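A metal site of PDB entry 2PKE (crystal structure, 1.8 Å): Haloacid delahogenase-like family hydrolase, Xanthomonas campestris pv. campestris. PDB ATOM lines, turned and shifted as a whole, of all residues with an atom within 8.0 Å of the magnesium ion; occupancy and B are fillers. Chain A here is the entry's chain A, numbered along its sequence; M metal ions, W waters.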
ATOM      1  N   PHE A  18      30.367  15.398 -22.988  1.00  0.00           N
ATOM      2  CA  PHE A  18      29.570  15.933 -24.046  1.00  0.00           C
ATOM      3  C   PHE A  18      29.856  15.160 -25.309  1.00  0.00           C
ATOM      4  O   PHE A  18      31.026  14.973 -25.667  1.00  0.00           O
ATOM      5  CB  PHE A  18      29.924  17.402 -24.310  1.00  0.00           C
ATOM      6  CG  PHE A  18      29.583  18.319 -23.167  1.00  0.00           C
ATOM      7  CD1 PHE A  18      30.429  18.457 -22.098  1.00  0.00           C
ATOM      8  CD2 PHE A  18      28.389  19.014 -23.165  1.00  0.00           C
ATOM      9  CE1 PHE A  18      30.088  19.317 -21.039  1.00  0.00           C
ATOM     10  CE2 PHE A  18      28.074  19.856 -22.131  1.00  0.00           C
ATOM     11  CZ  PHE A  18      28.944  19.997 -21.068  1.00  0.00           C
ATOM     12  N   ASP A  19      28.826  14.788 -26.042  1.00  0.00           N
ATOM     13  CA  ASP A  19      28.982  14.415 -27.456  1.00  0.00           C
ATOM     14  C   ASP A  19      29.322  15.656 -28.306  1.00  0.00           C
ATOM     15  O   ASP A  19      29.160  16.809 -27.874  1.00  0.00           O
ATOM     16  CB  ASP A  19      27.675  13.775 -27.943  1.00  0.00           C
ATOM     17  CG  ASP A  19      27.701  13.356 -29.394  1.00  0.00           C
ATOM     18  OD1 ASP A  19      28.718  12.773 -29.866  1.00  0.00           O
ATOM     19  OD2 ASP A  19      26.677  13.593 -30.111  1.00  0.00           O
ATOM     20  N   GLY A  20      29.841  15.446 -29.509  1.00  0.00           N
ATOM     21  CA  GLY A  20      30.087  16.611 -30.391  1.00  0.00           C
ATOM     22  C   GLY A  20      29.018  16.779 -31.466  1.00  0.00           C
ATOM     23  O   GLY A  20      28.191  17.688 -31.427  1.00  0.00           O
ATOM     24  N   ASP A  21      29.067  15.899 -32.448  1.00  0.00           N
ATOM     25  CA  ASP A  21      28.216  16.012 -33.643  1.00  0.00           C
ATOM     26  C   ASP A  21      26.750  15.995 -33.249  1.00  0.00           C
ATOM     27  O   ASP A  21      26.270  15.073 -32.561  1.00  0.00           O
ATOM     28  CB  ASP A  21      28.454  14.817 -34.582  1.00  0.00           C
ATOM     29  CG  ASP A  21      29.798  14.830 -35.309  1.00  0.00           C
ATOM     30  OD1 ASP A  21      30.440  15.851 -35.541  1.00  0.00           O
ATOM     31  OD2 ASP A  21      30.207  13.744 -35.762  1.00  0.00           O
ATOM     32  N   ASP A  22      26.054  17.072 -33.581  1.00  0.00           N
ATOM     33  CA  ASP A  22      24.625  17.219 -33.359  1.00  0.00           C
ATOM     34  C   ASP A  22      24.244  17.442 -31.896  1.00  0.00           C
ATOM     35  O   ASP A  22      23.044  17.372 -31.558  1.00  0.00           O
ATOM     36  CB  ASP A  22      23.865  16.039 -33.942  1.00  0.00           C
ATOM     37  CG  ASP A  22      24.278  15.742 -35.348  1.00  0.00           C
ATOM     38  OD1 ASP A  22      24.209  16.672 -36.174  1.00  0.00           O
ATOM     39  OD2 ASP A  22      24.749  14.609 -35.576  1.00  0.00           O
ATOM     40  N   THR A  23      25.253  17.731 -31.081  1.00  0.00           N
ATOM     41  CA  THR A  23      25.104  18.069 -29.665  1.00  0.00           C
ATOM     42  C   THR A  23      25.747  19.471 -29.409  1.00  0.00           C
ATOM     43  O   THR A  23      25.062  20.411 -28.958  1.00  0.00           O
ATOM     44  CB  THR A  23      25.735  17.009 -28.719  1.00  0.00           C
ATOM     45  OG1 THR A  23      25.046  15.759 -28.856  1.00  0.00           O
ATOM     46  CG2 THR A  23      25.655  17.498 -27.272  1.00  0.00           C
ATOM     47  N   LEU A  24      27.046  19.588 -29.702  1.00  0.00           N
ATOM     48  CA  LEU A  24      27.763  20.876 -29.616  1.00  0.00           C
ATOM     49  C   LEU A  24      27.721  21.673 -30.931  1.00  0.00           C
ATOM     50  O   LEU A  24      27.756  22.901 -30.916  1.00  0.00           O
ATOM     51  CB  LEU A  24      29.215  20.681 -29.182  1.00  0.00           C
ATOM     52  CG  LEU A  24      29.473  19.921 -27.873  1.00  0.00           C
ATOM     53  CD1 LEU A  24      30.966  19.691 -27.763  1.00  0.00           C
ATOM     54  CD2 LEU A  24      28.945  20.689 -26.705  1.00  0.00           C
ATOM     55  N   TRP A  25      27.706  20.991 -32.075  1.00  0.00           N
ATOM     56  CA  TRP A  25      27.743  21.674 -33.368  1.00  0.00           C
ATOM     57  C   TRP A  25      26.879  20.878 -34.336  1.00  0.00           C
ATOM     58  O   TRP A  25      26.567  19.727 -34.086  1.00  0.00           O
ATOM     59  CB  TRP A  25      29.217  21.809 -33.904  1.00  0.00           C
ATOM     60  CG  TRP A  25      29.993  20.530 -33.898  1.00  0.00           C
ATOM     61  CD1 TRP A  25      29.774  19.451 -34.705  1.00  0.00           C
ATOM     62  CD2 TRP A  25      31.061  20.157 -33.020  1.00  0.00           C
ATOM     63  NE1 TRP A  25      30.637  18.455 -34.417  1.00  0.00           N
ATOM     64  CE2 TRP A  25      31.455  18.852 -33.390  1.00  0.00           C
ATOM     65  CE3 TRP A  25      31.751  20.815 -31.991  1.00  0.00           C
ATOM     66  CZ2 TRP A  25      32.483  18.160 -32.743  1.00  0.00           C
ATOM     67  CZ3 TRP A  25      32.781  20.147 -31.363  1.00  0.00           C
ATOM     68  CH2 TRP A  25      33.124  18.829 -31.720  1.00  0.00           C
ATOM     69  N   SER A  27      26.119  18.728 -37.633  1.00  0.00           N
ATOM     70  CA  SER A  27      26.857  17.696 -38.379  1.00  0.00           C
ATOM     71  C   SER A  27      25.955  16.976 -39.351  1.00  0.00           C
ATOM     72  O   SER A  27      26.281  16.821 -40.500  1.00  0.00           O
ATOM     73  CB  SER A  27      27.428  16.657 -37.423  1.00  0.00           C
ATOM     74  OG  SER A  27      28.044  15.617 -38.135  1.00  0.00           O
ATOM     75  N   GLU A  28      24.831  16.530 -38.843  1.00  0.00           N
ATOM     76  CA  GLU A  28      23.914  15.756 -39.634  1.00  0.00           C
ATOM     77  C   GLU A  28      23.443  16.514 -40.874  1.00  0.00           C
ATOM     78  O   GLU A  28      23.241  15.931 -41.904  1.00  0.00           O
ATOM     79  CB  GLU A  28      22.696  15.352 -38.791  1.00  0.00           C
ATOM     80  CG  GLU A  28      21.869  14.287 -39.466  1.00  0.00           C
ATOM     81  CD  GLU A  28      22.639  12.964 -39.703  1.00  0.00           C
ATOM     82  OE1 GLU A  28      23.562  12.611 -38.904  1.00  0.00           O
ATOM     83  OE2 GLU A  28      22.320  12.260 -40.700  1.00  0.00           O
ATOM     84  N   ILE A 133      33.424  13.457 -25.562  1.00  0.00           N
ATOM     85  CA  ILE A 133      33.573  12.049 -25.917  1.00  0.00           C
ATOM     86  C   ILE A 133      32.824  11.832 -27.190  1.00  0.00           C
ATOM     87  O   ILE A 133      31.580  12.020 -27.285  1.00  0.00           O
ATOM     88  CB  ILE A 133      33.087  11.095 -24.825  1.00  0.00           C
ATOM     89  CG1 ILE A 133      33.819  11.426 -23.530  1.00  0.00           C
ATOM     90  CG2 ILE A 133      33.269   9.596 -25.241  1.00  0.00           C
ATOM     91  CD1 ILE A 133      33.371  10.648 -22.259  1.00  0.00           C
ATOM     92  N   THR A 134      33.557  11.410 -28.194  1.00  0.00           N
ATOM     93  CA  THR A 134      32.950  11.124 -29.486  1.00  0.00           C
ATOM     94  C   THR A 134      33.504   9.873 -30.182  1.00  0.00           C
ATOM     95  O   THR A 134      34.588   9.469 -29.883  1.00  0.00           O
ATOM     96  CB  THR A 134      33.139  12.307 -30.443  1.00  0.00           C
ATOM     97  OG1 THR A 134      32.280  12.067 -31.577  1.00  0.00           O
ATOM     98  CG2 THR A 134      34.580  12.400 -30.911  1.00  0.00           C
ATOM     99  N   LYS A 135      32.707   9.230 -31.033  1.00  0.00           N
ATOM    100  CA  LYS A 135      33.197   8.134 -31.832  1.00  0.00           C
ATOM    101  C   LYS A 135      33.501   8.629 -33.236  1.00  0.00           C
ATOM    102  O   LYS A 135      33.101   9.733 -33.624  1.00  0.00           O
ATOM    103  CB  LYS A 135      32.240   6.925 -31.837  1.00  0.00           C
ATOM    104  CG  LYS A 135      30.981   7.051 -32.629  1.00  0.00           C
ATOM    105  CD  LYS A 135      29.978   5.976 -32.181  1.00  0.00           C
ATOM    106  CE  LYS A 135      28.742   6.004 -32.978  1.00  0.00           C
ATOM    107  NZ  LYS A 135      27.893   4.876 -32.498  1.00  0.00           N
ATOM    108  N   LYS A 163      30.855   3.668 -29.085  1.00  0.00           N
ATOM    109  CA  LYS A 163      30.273   4.132 -27.824  1.00  0.00           C
ATOM    110  C   LYS A 163      29.421   2.981 -27.239  1.00  0.00           C
ATOM    111  O   LYS A 163      28.311   2.765 -27.625  1.00  0.00           O
ATOM    112  CB  LYS A 163      29.417   5.366 -28.048  1.00  0.00           C
ATOM    113  CG  LYS A 163      30.211   6.676 -27.909  1.00  0.00           C
ATOM    114  CD  LYS A 163      29.309   7.885 -28.170  1.00  0.00           C
ATOM    115  CE  LYS A 163      30.015   9.182 -27.908  1.00  0.00           C
ATOM    116  NZ  LYS A 163      29.226  10.332 -28.475  1.00  0.00           N
ATOM    117  N   MET A 184      26.570  12.101 -18.926  1.00  0.00           N
ATOM    118  CA  MET A 184      26.881  12.238 -20.351  1.00  0.00           C
ATOM    119  C   MET A 184      25.748  12.990 -21.063  1.00  0.00           C
ATOM    120  O   MET A 184      24.570  12.630 -20.869  1.00  0.00           O
ATOM    121  CB  MET A 184      27.077  10.872 -20.978  1.00  0.00           C
ATOM    122  CG  MET A 184      27.329  10.943 -22.495  1.00  0.00           C
ATOM    123  SD  MET A 184      29.053  11.630 -23.066  1.00  0.00           S
ATOM    124  CE  MET A 184      28.549  11.371 -24.922  1.00  0.00           C
ATOM    125  N   ILE A 185      26.130  13.993 -21.888  1.00  0.00           N
ATOM    126  CA  ILE A 185      25.155  14.799 -22.657  1.00  0.00           C
ATOM    127  C   ILE A 185      25.292  14.474 -24.129  1.00  0.00           C
ATOM    128  O   ILE A 185      26.373  14.544 -24.683  1.00  0.00           O
ATOM    129  CB  ILE A 185      25.337  16.317 -22.462  1.00  0.00           C
ATOM    130  CG1 ILE A 185      25.250  16.701 -20.976  1.00  0.00           C
ATOM    131  CG2 ILE A 185      24.286  17.094 -23.297  1.00  0.00           C
ATOM    132  CD1 ILE A 185      25.398  18.178 -20.713  1.00  0.00           C
ATOM    133  N   GLY A 186      24.183  14.079 -24.756  1.00  0.00           N
ATOM    134  CA  GLY A 186      24.207  13.827 -26.182  1.00  0.00           C
ATOM    135  C   GLY A 186      22.864  13.751 -26.872  1.00  0.00           C
ATOM    136  O   GLY A 186      21.811  13.790 -26.253  1.00  0.00           O
ATOM    137  N   ASN A 187      22.909  13.641 -28.186  1.00  0.00           N
ATOM    138  CA  ASN A 187      21.708  13.631 -28.997  1.00  0.00           C
ATOM    139  C   ASN A 187      21.201  12.263 -29.376  1.00  0.00           C
ATOM    140  O   ASN A 187      20.127  12.171 -29.948  1.00  0.00           O
ATOM    141  CB  ASN A 187      21.917  14.425 -30.284  1.00  0.00           C
ATOM    142  CG  ASN A 187      22.908  13.764 -31.234  1.00  0.00           C
ATOM    143  OD1 ASN A 187      24.111  13.820 -31.008  1.00  0.00           O
ATOM    144  ND2 ASN A 187      22.393  13.167 -32.320  1.00  0.00           N
ATOM    145  N   SER A 188      21.997  11.217 -29.119  1.00  0.00           N
ATOM    146  CA  SER A 188      21.602   9.824 -29.455  1.00  0.00           C
ATOM    147  C   SER A 188      21.384   9.019 -28.173  1.00  0.00           C
ATOM    148  O   SER A 188      22.309   8.838 -27.416  1.00  0.00           O
ATOM    149  CB  SER A 188      22.700   9.172 -30.308  1.00  0.00           C
ATOM    150  OG  SER A 188      22.449   7.791 -30.463  1.00  0.00           O
ATOM    151  N   SER A 191      23.576   5.748 -28.475  1.00  0.00           N
ATOM    152  CA  SER A 191      25.039   5.903 -28.323  1.00  0.00           C
ATOM    153  C   SER A 191      25.507   6.729 -27.147  1.00  0.00           C
ATOM    154  O   SER A 191      26.584   6.485 -26.599  1.00  0.00           O
ATOM    155  CB  SER A 191      25.638   6.530 -29.586  1.00  0.00           C
ATOM    156  OG  SER A 191      25.652   5.583 -30.591  1.00  0.00           O
ATOM    157  N   ASP A 192      24.768   7.782 -26.808  1.00  0.00           N
ATOM    158  CA  ASP A 192      25.240   8.721 -25.844  1.00  0.00           C
ATOM    159  C   ASP A 192      24.708   8.377 -24.446  1.00  0.00           C
ATOM    160  O   ASP A 192      25.447   8.368 -23.481  1.00  0.00           O
ATOM    161  CB  ASP A 192      24.885  10.162 -26.278  1.00  0.00           C
ATOM    162  CG  ASP A 192      25.543  10.547 -27.599  1.00  0.00           C
ATOM    163  OD1 ASP A 192      26.739  10.192 -27.777  1.00  0.00           O
ATOM    164  OD2 ASP A 192      24.903  11.184 -28.466  1.00  0.00           O
ATOM    165  N   THR A 206      19.352  15.296 -25.507  1.00  0.00           N
ATOM    166  CA  THR A 206      18.945  16.465 -26.309  1.00  0.00           C
ATOM    167  C   THR A 206      18.913  16.093 -27.793  1.00  0.00           C
ATOM    168  O   THR A 206      19.919  16.209 -28.502  1.00  0.00           O
ATOM    169  CB  THR A 206      19.883  17.640 -26.101  1.00  0.00           C
ATOM    170  OG1 THR A 206      19.822  18.026 -24.729  1.00  0.00           O
ATOM    171  CG2 THR A 206      19.462  18.859 -26.928  1.00  0.00           C
ATOM    172  N   TYR A 208      18.479  16.016 -31.803  1.00  0.00           N
ATOM    173  CA  TYR A 208      18.744  17.004 -32.828  1.00  0.00           C
ATOM    174  C   TYR A 208      17.639  16.901 -33.854  1.00  0.00           C
ATOM    175  O   TYR A 208      17.408  15.818 -34.383  1.00  0.00           O
ATOM    176  CB  TYR A 208      20.087  16.721 -33.488  1.00  0.00           C
ATOM    177  CG  TYR A 208      20.513  17.819 -34.436  1.00  0.00           C
ATOM    178  CD1 TYR A 208      20.886  19.071 -33.942  1.00  0.00           C
ATOM    179  CD2 TYR A 208      20.542  17.612 -35.804  1.00  0.00           C
ATOM    180  CE1 TYR A 208      21.260  20.080 -34.788  1.00  0.00           C
ATOM    181  CE2 TYR A 208      20.930  18.620 -36.670  1.00  0.00           C
ATOM    182  CZ  TYR A 208      21.285  19.856 -36.148  1.00  0.00           C
ATOM    183  OH  TYR A 208      21.686  20.875 -36.977  1.00  0.00           O
HETATM  184 MG    MG M   1      25.885  13.170 -31.884  1.00  0.00          MG
HETATM  185  O   HOH W   1      25.318  11.249 -31.020  1.00  0.00           O
HETATM  186  O   HOH W   2      27.845  12.371 -32.262  1.00  0.00           O
HETATM  187  O   HOH W   3      24.932  12.772 -33.678  1.00  0.00           O
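The side-chain carboxylate (OD2) of Asp 19 sits close to the side-chain hydroxyl (OG1) of Thr 23, 3.0 Å away.
The side-chain carboxylate (OD1) of Asp 19 is in salt-bridge range of the side-chain amino group (NZ) of Lys 163 (2.9 Å).
N of Asp 19 sits at hydrogen-bond distance from O of Ile 185 (2.8 Å).
The side-chain carboxylate (OD1) of Asp 21 lies within hydrogen-bond range of the indole nitrogen (NE1) of Trp 25.
N of Asn 187 lies within hydrogen-bond range of OG1 of Thr 23 (3.1 Å).
The backbone NH (N) of Asn 187 sits at hydrogen-bond distance from the side-chain carboxylate (OD2) of Asp 192, 3.2 Å away.
The nearest printed residue that does not touch the magnesium ion is Asp 22 (4.1 Å).
The magnesium ion is bound by OD2 of Asp 19, O of Asp 21, water W3, OD1 of Asn 187, water W2 and water W1.
Water W3 bridges OD2 of Asp 22 (2.6 Å) and ND2 of Asn 187 (2.9 Å).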
